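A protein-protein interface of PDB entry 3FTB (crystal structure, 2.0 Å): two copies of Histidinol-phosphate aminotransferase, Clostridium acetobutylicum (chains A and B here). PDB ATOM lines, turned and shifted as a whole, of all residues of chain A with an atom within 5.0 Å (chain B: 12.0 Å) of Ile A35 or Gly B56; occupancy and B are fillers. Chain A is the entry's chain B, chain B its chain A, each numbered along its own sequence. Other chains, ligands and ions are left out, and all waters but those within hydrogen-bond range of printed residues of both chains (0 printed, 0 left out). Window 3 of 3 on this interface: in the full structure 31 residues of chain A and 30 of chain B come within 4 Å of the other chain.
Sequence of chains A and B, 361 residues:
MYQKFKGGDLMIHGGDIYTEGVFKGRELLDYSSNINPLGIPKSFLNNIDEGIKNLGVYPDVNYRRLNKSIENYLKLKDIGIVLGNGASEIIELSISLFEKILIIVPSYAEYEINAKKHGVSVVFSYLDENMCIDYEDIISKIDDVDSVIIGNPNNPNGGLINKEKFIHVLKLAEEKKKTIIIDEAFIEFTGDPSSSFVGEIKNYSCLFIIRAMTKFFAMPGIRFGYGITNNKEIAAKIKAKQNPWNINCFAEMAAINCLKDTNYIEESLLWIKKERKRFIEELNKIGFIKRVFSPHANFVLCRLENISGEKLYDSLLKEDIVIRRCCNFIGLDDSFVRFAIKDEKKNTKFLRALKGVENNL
No position is printed for both chains.
Hydrophobic or aromatic side chains of chain A that line the printed part of chain B: Ile A35 and Pro A220.
Hydrophobic or aromatic side chains of chain B within 4 Å of the printed part of chain A: Tyr B58.
Among the printed residues, 10 pairs touch across the chains.
The side-chain hydroxyl (OH) of Tyr B58 sits at hydrogen-bond distance from the side-chain amino group (NZ) of Lys A215.
N of Pro A220 lies close to O of Leu B55, at 3.1 Å.
The backbone carbonyl oxygen (O) of Lys A215 is in hydrogen-bond range of the backbone NH (N) of Asn A36 (2.7 Å).
N of Met A219 sits at hydrogen-bond distance from O of Thr A214 (3.3 Å).
No residue of chain B comes within 4 Å of Asn A34.
No residue of chain B comes within 4 Å of Asn A36.
Thr A214 touches just one residue of chain B: Tyr B58.
Lys A215 touches just one residue of chain B: Tyr B58 (3.3 Å).
Printed residues of chain B within 4 Å of Met A219: Leu B55 (3.3 Å).
Pro A220 touches just these residues of chain B: Leu B55, Gly B56, Val B57 and Tyr B58.
Asn B54 touches none of the printed residues of chain A.
Of the printed residues of chain A, Leu B55 touches Ala A218, Met A219 and Pro A220.
Printed residues of chain A within 4 Å of Gly B56: Ile A35, Ala A218 and Pro A220.
Of the printed residues of chain A, Val B57 touches Pro A220.
Of the printed residues of chain A, Tyr B58 touches Thr A214, Lys A215 and Pro A220.
Pro B59 touches none of the printed residues of chain A.
The nearest residue of chain A that does not touch Gly B56 is Ile A40 (4.7 Å).
Ile A35 touches Gly B56.
Tyr B58 touches Thr A214.
Leu B55 touches Ala A218.
O of Ala A218 touches CA of Gly B56 (3.7 Å).
Met A219 touches Leu B55 (CA to O, 3.3 Å).
CG of Pro A220 touches O of Gly B56 (3.5 Å).
C of Val B57 touches CB of Pro A220 (3.8 Å).
CB of Pro A220 touches N of Tyr B58, 3.8 Å away.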
ATOM      1  N   SER A  33      11.318  15.448 -27.074  1.00  0.00           N
ATOM      2  CA  SER A  33      11.147  16.901 -27.156  1.00  0.00           C
ATOM      3  C   SER A  33      12.254  17.661 -26.434  1.00  0.00           C
ATOM      4  O   SER A  33      12.552  17.382 -25.272  1.00  0.00           O
ATOM      5  CB  SER A  33       9.790  17.323 -26.594  1.00  0.00           C
ATOM      6  OG  SER A  33       9.775  18.721 -26.342  1.00  0.00           O
ATOM      7  N   ASN A  34      12.838  18.640 -27.122  1.00  0.00           N
ATOM      8  CA  ASN A  34      14.014  19.342 -26.612  1.00  0.00           C
ATOM      9  C   ASN A  34      13.791  20.800 -26.151  1.00  0.00           C
ATOM     10  O   ASN A  34      14.610  21.682 -26.400  1.00  0.00           O
ATOM     11  CB  ASN A  34      15.138  19.283 -27.645  1.00  0.00           C
ATOM     12  CG  ASN A  34      15.584  17.868 -27.951  1.00  0.00           C
ATOM     13  OD1 ASN A  34      15.892  17.549 -29.097  1.00  0.00           O
ATOM     14  ND2 ASN A  34      15.629  17.017 -26.937  1.00  0.00           N
ATOM     15  N   ILE A  35      12.695  21.035 -25.441  1.00  0.00           N
ATOM     16  CA  ILE A  35      12.397  22.356 -24.911  1.00  0.00           C
ATOM     17  C   ILE A  35      13.096  22.568 -23.569  1.00  0.00           C
ATOM     18  O   ILE A  35      13.086  21.683 -22.721  1.00  0.00           O
ATOM     19  CB  ILE A  35      10.871  22.546 -24.749  1.00  0.00           C
ATOM     20  CG1 ILE A  35      10.155  22.139 -26.040  1.00  0.00           C
ATOM     21  CG2 ILE A  35      10.533  24.001 -24.409  1.00  0.00           C
ATOM     22  CD1 ILE A  35      10.735  22.811 -27.266  1.00  0.00           C
ATOM     23  N   ASN A  36      13.711  23.737 -23.387  1.00  0.00           N
ATOM     24  CA  ASN A  36      14.303  24.106 -22.094  1.00  0.00           C
ATOM     25  C   ASN A  36      13.329  23.781 -20.950  1.00  0.00           C
ATOM     26  O   ASN A  36      12.182  24.244 -20.951  1.00  0.00           O
ATOM     27  CB  ASN A  36      14.700  25.596 -22.086  1.00  0.00           C
ATOM     28  CG  ASN A  36      15.378  26.019 -20.796  1.00  0.00           C
ATOM     29  OD1 ASN A  36      15.119  25.459 -19.738  1.00  0.00           O
ATOM     30  ND2 ASN A  36      16.253  27.012 -20.880  1.00  0.00           N
ATOM     31  N   PRO A  37      13.776  22.947 -19.997  1.00  0.00           N
ATOM     32  CA  PRO A  37      13.006  22.358 -18.888  1.00  0.00           C
ATOM     33  C   PRO A  37      12.719  23.289 -17.716  1.00  0.00           C
ATOM     34  O   PRO A  37      11.910  22.930 -16.863  1.00  0.00           O
ATOM     35  CB  PRO A  37      13.910  21.212 -18.403  1.00  0.00           C
ATOM     36  CG  PRO A  37      14.855  20.955 -19.520  1.00  0.00           C
ATOM     37  CD  PRO A  37      15.090  22.307 -20.124  1.00  0.00           C
ATOM     38  N   ILE A  40       8.812  28.792 -18.437  1.00  0.00           N
ATOM     39  CA  ILE A  40       8.747  30.148 -18.980  1.00  0.00           C
ATOM     40  C   ILE A  40       9.652  31.116 -18.199  1.00  0.00           C
ATOM     41  O   ILE A  40       9.777  31.006 -16.977  1.00  0.00           O
ATOM     42  CB  ILE A  40       7.281  30.650 -18.976  1.00  0.00           C
ATOM     43  CG1 ILE A  40       6.424  29.718 -19.833  1.00  0.00           C
ATOM     44  CG2 ILE A  40       7.172  32.085 -19.455  1.00  0.00           C
ATOM     45  CD1 ILE A  40       7.160  29.154 -21.044  1.00  0.00           C
ATOM     46  N   THR A 214      12.020  29.229 -29.277  1.00  0.00           N
ATOM     47  CA  THR A 214      11.278  28.011 -28.976  1.00  0.00           C
ATOM     48  C   THR A 214      11.998  27.110 -27.965  1.00  0.00           C
ATOM     49  O   THR A 214      11.467  26.758 -26.914  1.00  0.00           O
ATOM     50  CB  THR A 214      11.044  27.224 -30.283  1.00  0.00           C
ATOM     51  OG1 THR A 214      10.559  28.115 -31.298  1.00  0.00           O
ATOM     52  CG2 THR A 214      10.053  26.090 -30.077  1.00  0.00           C
ATOM     53  N   LYS A 215      13.221  26.742 -28.300  1.00  0.00           N
ATOM     54  CA  LYS A 215      13.951  25.751 -27.540  1.00  0.00           C
ATOM     55  C   LYS A 215      14.430  26.289 -26.204  1.00  0.00           C
ATOM     56  O   LYS A 215      14.010  25.822 -25.150  1.00  0.00           O
ATOM     57  CB  LYS A 215      15.128  25.238 -28.379  1.00  0.00           C
ATOM     58  CG  LYS A 215      14.688  24.616 -29.709  1.00  0.00           C
ATOM     59  CD  LYS A 215      13.456  23.717 -29.491  1.00  0.00           C
ATOM     60  CE  LYS A 215      13.205  22.709 -30.624  1.00  0.00           C
ATOM     61  NZ  LYS A 215      12.894  23.391 -31.902  1.00  0.00           N
ATOM     62  N   ALA A 218      11.909  28.350 -23.922  1.00  0.00           N
ATOM     63  CA  ALA A 218      10.825  27.423 -23.541  1.00  0.00           C
ATOM     64  C   ALA A 218       9.399  27.814 -23.957  1.00  0.00           C
ATOM     65  O   ALA A 218       8.433  27.552 -23.227  1.00  0.00           O
ATOM     66  CB  ALA A 218      10.882  27.124 -22.041  1.00  0.00           C
ATOM     67  N   MET A 219       9.256  28.424 -25.133  1.00  0.00           N
ATOM     68  CA  MET A 219       7.944  28.916 -25.565  1.00  0.00           C
ATOM     69  C   MET A 219       7.583  28.518 -27.009  1.00  0.00           C
ATOM     70  O   MET A 219       7.474  29.378 -27.882  1.00  0.00           O
ATOM     71  CB  MET A 219       7.851  30.448 -25.387  1.00  0.00           C
ATOM     72  CG  MET A 219       7.603  30.919 -23.939  1.00  0.00           C
ATOM     73  SD  MET A 219       7.792  32.709 -23.670  1.00  0.00           S
ATOM     74  CE  MET A 219       9.091  33.043 -24.874  1.00  0.00           C
ATOM     75  N   PRO A 220       7.386  27.212 -27.262  1.00  0.00           N
ATOM     76  CA  PRO A 220       7.009  26.746 -28.605  1.00  0.00           C
ATOM     77  C   PRO A 220       5.664  27.319 -29.078  1.00  0.00           C
ATOM     78  O   PRO A 220       5.539  27.757 -30.232  1.00  0.00           O
ATOM     79  CB  PRO A 220       6.892  25.224 -28.439  1.00  0.00           C
ATOM     80  CG  PRO A 220       7.619  24.896 -27.178  1.00  0.00           C
ATOM     81  CD  PRO A 220       7.512  26.104 -26.299  1.00  0.00           C
ATOM     82  N   ASN A 298      21.153  20.559 -25.317  1.00  0.00           N
ATOM     83  CA  ASN A 298      20.314  19.797 -24.409  1.00  0.00           C
ATOM     84  C   ASN A 298      19.705  18.531 -25.040  1.00  0.00           C
ATOM     85  O   ASN A 298      18.575  18.150 -24.706  1.00  0.00           O
ATOM     86  CB  ASN A 298      19.175  20.688 -23.928  1.00  0.00           C
ATOM     87  CG  ASN A 298      18.225  21.053 -25.062  1.00  0.00           C
ATOM     88  OD1 ASN A 298      18.641  21.120 -26.222  1.00  0.00           O
ATOM     89  ND2 ASN A 298      16.951  21.257 -24.744  1.00  0.00           N
ATOM     90  N   ILE B  48      -6.959  32.636 -19.785  1.00  0.00           N
ATOM     91  CA  ILE B  48      -5.567  32.988 -20.045  1.00  0.00           C
ATOM     92  C   ILE B  48      -4.617  31.943 -19.457  1.00  0.00           C
ATOM     93  O   ILE B  48      -3.495  31.768 -19.941  1.00  0.00           O
ATOM     94  CB  ILE B  48      -5.224  34.371 -19.484  1.00  0.00           C
ATOM     95  CG1 ILE B  48      -3.828  34.796 -19.935  1.00  0.00           C
ATOM     96  CG2 ILE B  48      -5.322  34.368 -17.964  1.00  0.00           C
ATOM     97  CD1 ILE B  48      -3.696  34.972 -21.426  1.00  0.00           C
ATOM     98  N   ASP B  49      -5.073  31.247 -18.417  1.00  0.00           N
ATOM     99  CA  ASP B  49      -4.283  30.180 -17.811  1.00  0.00           C
ATOM    100  C   ASP B  49      -4.034  29.092 -18.839  1.00  0.00           C
ATOM    101  O   ASP B  49      -2.909  28.643 -19.022  1.00  0.00           O
ATOM    102  CB  ASP B  49      -5.011  29.583 -16.608  1.00  0.00           C
ATOM    103  CG  ASP B  49      -5.196  30.581 -15.481  1.00  0.00           C
ATOM    104  OD1 ASP B  49      -4.750  31.740 -15.626  1.00  0.00           O
ATOM    105  OD2 ASP B  49      -5.788  30.203 -14.446  1.00  0.00           O
ATOM    106  N   GLU B  50      -5.104  28.666 -19.498  1.00  0.00           N
ATOM    107  CA  GLU B  50      -5.018  27.675 -20.559  1.00  0.00           C
ATOM    108  C   GLU B  50      -3.931  28.074 -21.549  1.00  0.00           C
ATOM    109  O   GLU B  50      -3.030  27.290 -21.840  1.00  0.00           O
ATOM    110  CB  GLU B  50      -6.377  27.546 -21.260  1.00  0.00           C
ATOM    111  CG  GLU B  50      -6.372  26.725 -22.535  1.00  0.00           C
ATOM    112  CD  GLU B  50      -7.778  26.458 -23.063  1.00  0.00           C
ATOM    113  OE1 GLU B  50      -7.921  26.165 -24.273  1.00  0.00           O
ATOM    114  OE2 GLU B  50      -8.736  26.541 -22.265  1.00  0.00           O
ATOM    115  N   GLY B  51      -4.020  29.303 -22.055  1.00  0.00           N
ATOM    116  CA  GLY B  51      -3.044  29.828 -22.990  1.00  0.00           C
ATOM    117  C   GLY B  51      -1.608  29.760 -22.497  1.00  0.00           C
ATOM    118  O   GLY B  51      -0.738  29.247 -23.195  1.00  0.00           O
ATOM    119  N   ILE B  52      -1.353  30.281 -21.301  1.00  0.00           N
ATOM    120  CA  ILE B  52      -0.011  30.245 -20.715  1.00  0.00           C
ATOM    121  C   ILE B  52       0.551  28.831 -20.546  1.00  0.00           C
ATOM    122  O   ILE B  52       1.729  28.586 -20.804  1.00  0.00           O
ATOM    123  CB  ILE B  52       0.037  30.957 -19.354  1.00  0.00           C
ATOM    124  CG1 ILE B  52      -0.507  32.378 -19.482  1.00  0.00           C
ATOM    125  CG2 ILE B  52       1.468  30.998 -18.839  1.00  0.00           C
ATOM    126  CD1 ILE B  52      -0.449  33.159 -18.197  1.00  0.00           C
ATOM    127  N   LYS B  53      -0.295  27.904 -20.111  1.00  0.00           N
ATOM    128  CA  LYS B  53       0.123  26.516 -19.910  1.00  0.00           C
ATOM    129  C   LYS B  53       0.704  25.938 -21.191  1.00  0.00           C
ATOM    130  O   LYS B  53       1.800  25.374 -21.200  1.00  0.00           O
ATOM    131  CB  LYS B  53      -1.056  25.647 -19.456  1.00  0.00           C
ATOM    132  CG  LYS B  53      -0.651  24.262 -18.944  1.00  0.00           C
ATOM    133  CD  LYS B  53      -1.861  23.404 -18.572  1.00  0.00           C
ATOM    134  CE  LYS B  53      -2.096  22.277 -19.572  1.00  0.00           C
ATOM    135  NZ  LYS B  53      -1.164  21.126 -19.356  1.00  0.00           N
ATOM    136  N   ASN B  54      -0.048  26.081 -22.271  1.00  0.00           N
ATOM    137  CA  ASN B  54       0.340  25.517 -23.553  1.00  0.00           C
ATOM    138  C   ASN B  54       1.521  26.243 -24.198  1.00  0.00           C
ATOM    139  O   ASN B  54       2.001  25.831 -25.255  1.00  0.00           O
ATOM    140  CB  ASN B  54      -0.864  25.491 -24.495  1.00  0.00           C
ATOM    141  CG  ASN B  54      -2.060  24.745 -23.896  1.00  0.00           C
ATOM    142  OD1 ASN B  54      -1.913  23.675 -23.296  1.00  0.00           O
ATOM    143  ND2 ASN B  54      -3.246  25.310 -24.062  1.00  0.00           N
ATOM    144  N   LEU B  55       1.983  27.320 -23.563  1.00  0.00           N
ATOM    145  CA  LEU B  55       3.176  28.019 -24.036  1.00  0.00           C
ATOM    146  C   LEU B  55       4.331  27.050 -24.151  1.00  0.00           C
ATOM    147  O   LEU B  55       5.182  27.181 -25.033  1.00  0.00           O
ATOM    148  CB  LEU B  55       3.590  29.128 -23.070  1.00  0.00           C
ATOM    149  CG  LEU B  55       3.026  30.526 -23.287  1.00  0.00           C
ATOM    150  CD1 LEU B  55       3.613  31.456 -22.239  1.00  0.00           C
ATOM    151  CD2 LEU B  55       3.363  30.995 -24.685  1.00  0.00           C
ATOM    152  N   GLY B  56       4.355  26.086 -23.242  1.00  0.00           N
ATOM    153  CA  GLY B  56       5.506  25.224 -23.070  1.00  0.00           C
ATOM    154  C   GLY B  56       5.588  24.081 -24.055  1.00  0.00           C
ATOM    155  O   GLY B  56       6.624  23.409 -24.125  1.00  0.00           O
ATOM    156  N   VAL B  57       4.519  23.857 -24.820  1.00  0.00           N
ATOM    157  CA  VAL B  57       4.509  22.759 -25.786  1.00  0.00           C
ATOM    158  C   VAL B  57       3.968  23.156 -27.162  1.00  0.00           C
ATOM    159  O   VAL B  57       3.257  24.149 -27.302  1.00  0.00           O
ATOM    160  CB  VAL B  57       3.728  21.543 -25.250  1.00  0.00           C
ATOM    161  CG1 VAL B  57       4.334  21.089 -23.927  1.00  0.00           C
ATOM    162  CG2 VAL B  57       2.247  21.879 -25.090  1.00  0.00           C
ATOM    163  N   TYR B  58       4.329  22.376 -28.174  1.00  0.00           N
ATOM    164  CA  TYR B  58       3.785  22.541 -29.512  1.00  0.00           C
ATOM    165  C   TYR B  58       2.299  22.167 -29.533  1.00  0.00           C
ATOM    166  O   TYR B  58       1.898  21.143 -28.974  1.00  0.00           O
ATOM    167  CB  TYR B  58       4.544  21.653 -30.496  1.00  0.00           C
ATOM    168  CG  TYR B  58       5.903  22.186 -30.920  1.00  0.00           C
ATOM    169  CD1 TYR B  58       6.029  23.075 -31.985  1.00  0.00           C
ATOM    170  CD2 TYR B  58       7.062  21.770 -30.280  1.00  0.00           C
ATOM    171  CE1 TYR B  58       7.276  23.548 -32.383  1.00  0.00           C
ATOM    172  CE2 TYR B  58       8.309  22.235 -30.674  1.00  0.00           C
ATOM    173  CZ  TYR B  58       8.412  23.122 -31.721  1.00  0.00           C
ATOM    174  OH  TYR B  58       9.654  23.577 -32.103  1.00  0.00           O
ATOM    175  N   PRO B  59       1.476  22.993 -30.189  1.00  0.00           N
ATOM    176  CA  PRO B  59       0.056  22.655 -30.299  1.00  0.00           C
ATOM    177  C   PRO B  59      -0.082  21.366 -31.096  1.00  0.00           C
ATOM    178  O   PRO B  59       0.916  20.890 -31.643  1.00  0.00           O
ATOM    179  CB  PRO B  59      -0.521  23.815 -31.115  1.00  0.00           C
ATOM    180  CG  PRO B  59       0.544  24.896 -31.103  1.00  0.00           C
ATOM    181  CD  PRO B  59       1.839  24.189 -30.968  1.00  0.00           C
ATOM    182  N   ASP B  60      -1.290  20.814 -31.165  1.00  0.00           N
ATOM    183  CA  ASP B  60      -1.553  19.681 -32.043  1.00  0.00           C
ATOM    184  C   ASP B  60      -1.224  20.101 -33.466  1.00  0.00           C
ATOM    185  O   ASP B  60      -1.704  21.124 -33.929  1.00  0.00           O
ATOM    186  CB  ASP B  60      -3.020  19.250 -31.944  1.00  0.00           C
ATOM    187  CG  ASP B  60      -3.346  18.042 -32.829  1.00  0.00           C
ATOM    188  OD1 ASP B  60      -2.412  17.404 -33.366  1.00  0.00           O
ATOM    189  OD2 ASP B  60      -4.544  17.726 -32.983  1.00  0.00           O
ATOM    190  N   TRP B 245       2.189  24.089 -37.423  1.00  0.00           N
ATOM    191  CA  TRP B 245       2.088  25.025 -36.300  1.00  0.00           C
ATOM    192  C   TRP B 245       2.137  26.536 -36.634  1.00  0.00           C
ATOM    193  O   TRP B 245       2.800  27.297 -35.932  1.00  0.00           O
ATOM    194  CB  TRP B 245       3.148  24.697 -35.253  1.00  0.00           C
ATOM    195  CG  TRP B 245       3.153  23.271 -34.864  1.00  0.00           C
ATOM    196  CD1 TRP B 245       2.245  22.633 -34.069  1.00  0.00           C
ATOM    197  CD2 TRP B 245       4.117  22.283 -35.247  1.00  0.00           C
ATOM    198  NE1 TRP B 245       2.585  21.307 -33.937  1.00  0.00           N
ATOM    199  CE2 TRP B 245       3.732  21.070 -34.648  1.00  0.00           C
ATOM    200  CE3 TRP B 245       5.273  22.310 -36.035  1.00  0.00           C
ATOM    201  CZ2 TRP B 245       4.458  19.891 -34.816  1.00  0.00           C
ATOM    202  CZ3 TRP B 245       5.987  21.138 -36.204  1.00  0.00           C
ATOM    203  CH2 TRP B 245       5.580  19.947 -35.598  1.00  0.00           C
ATOM    204  N   ILE B 247      -0.134  28.566 -36.129  1.00  0.00           N
ATOM    205  CA  ILE B 247      -1.079  29.211 -35.218  1.00  0.00           C
ATOM    206  C   ILE B 247      -0.562  29.171 -33.787  1.00  0.00           C
ATOM    207  O   ILE B 247      -0.481  28.112 -33.192  1.00  0.00           O
ATOM    208  CB  ILE B 247      -2.464  28.508 -35.269  1.00  0.00           C
ATOM    209  CG1 ILE B 247      -2.979  28.430 -36.704  1.00  0.00           C
ATOM    210  CG2 ILE B 247      -3.482  29.189 -34.365  1.00  0.00           C
ATOM    211  CD1 ILE B 247      -2.946  29.750 -37.435  1.00  0.00           C
ATOM    212  N   ASN B 248      -0.206  30.324 -33.235  1.00  0.00           N
ATOM    213  CA  ASN B 248       0.265  30.389 -31.847  1.00  0.00           C
ATOM    214  C   ASN B 248      -0.797  29.931 -30.839  1.00  0.00           C
ATOM    215  O   ASN B 248      -1.987  29.893 -31.154  1.00  0.00           O
ATOM    216  CB  ASN B 248       0.730  31.805 -31.506  1.00  0.00           C
ATOM    217  CG  ASN B 248      -0.431  32.747 -31.219  1.00  0.00           C
ATOM    218  OD1 ASN B 248      -0.839  33.524 -32.081  1.00  0.00           O
ATOM    219  ND2 ASN B 248      -0.962  32.686 -30.004  1.00  0.00           N
ATOM    220  N   CYS B 249      -0.366  29.608 -29.620  1.00  0.00           N
ATOM    221  CA  CYS B 249      -1.251  29.002 -28.625  1.00  0.00           C
ATOM    222  C   CYS B 249      -2.379  29.904 -28.091  1.00  0.00           C
ATOM    223  O   CYS B 249      -3.463  29.411 -27.759  1.00  0.00           O
ATOM    224  CB  CYS B 249      -0.439  28.398 -27.465  1.00  0.00           C
ATOM    225  SG  CYS B 249       0.399  29.563 -26.345  1.00  0.00           S
ATOM    226  N   PHE B 250      -2.133  31.207 -27.997  1.00  0.00           N
ATOM    227  CA  PHE B 250      -3.163  32.139 -27.528  1.00  0.00           C
ATOM    228  C   PHE B 250      -4.264  32.279 -28.576  1.00  0.00           C
ATOM    229  O   PHE B 250      -5.460  32.263 -28.257  1.00  0.00           O
ATOM    230  CB  PHE B 250      -2.554  33.502 -27.200  1.00  0.00           C
ATOM    231  CG  PHE B 250      -1.607  33.473 -26.035  1.00  0.00           C
ATOM    232  CD1 PHE B 250      -2.089  33.419 -24.735  1.00  0.00           C
ATOM    233  CD2 PHE B 250      -0.232  33.498 -26.235  1.00  0.00           C
ATOM    234  CE1 PHE B 250      -1.213  33.392 -23.661  1.00  0.00           C
ATOM    235  CE2 PHE B 250       0.641  33.467 -25.162  1.00  0.00           C
ATOM    236  CZ  PHE B 250       0.148  33.410 -23.874  1.00  0.00           C
ATOM    237  N   GLU B 252      -5.058  30.047 -30.665  1.00  0.00           N
ATOM    238  CA  GLU B 252      -5.803  28.807 -30.486  1.00  0.00           C
ATOM    239  C   GLU B 252      -6.759  28.911 -29.306  1.00  0.00           C
ATOM    240  O   GLU B 252      -7.921  28.514 -29.411  1.00  0.00           O
ATOM    241  CB  GLU B 252      -4.843  27.642 -30.279  1.00  0.00           C
ATOM    242  CG  GLU B 252      -5.501  26.301 -30.159  1.00  0.00           C
ATOM    243  CD  GLU B 252      -4.492  25.195 -29.925  1.00  0.00           C
ATOM    244  OE1 GLU B 252      -3.580  25.390 -29.093  1.00  0.00           O
ATOM    245  OE2 GLU B 252      -4.605  24.134 -30.573  1.00  0.00           O
ATOM    246  N   MET B 253      -6.270  29.453 -28.190  1.00  0.00           N
ATOM    247  CA  MET B 253      -7.094  29.598 -26.993  1.00  0.00           C
ATOM    248  C   MET B 253      -8.300  30.501 -27.234  1.00  0.00           C
ATOM    249  O   MET B 253      -9.390  30.236 -26.720  1.00  0.00           O
ATOM    250  CB  MET B 253      -6.278  30.109 -25.803  1.00  0.00           C
ATOM    251  CG  MET B 253      -7.111  30.239 -24.528  1.00  0.00           C
ATOM    252  SD  MET B 253      -7.944  31.836 -24.332  1.00  0.00           S
ATOM    253  CE  MET B 253      -6.546  32.775 -23.705  1.00  0.00           C
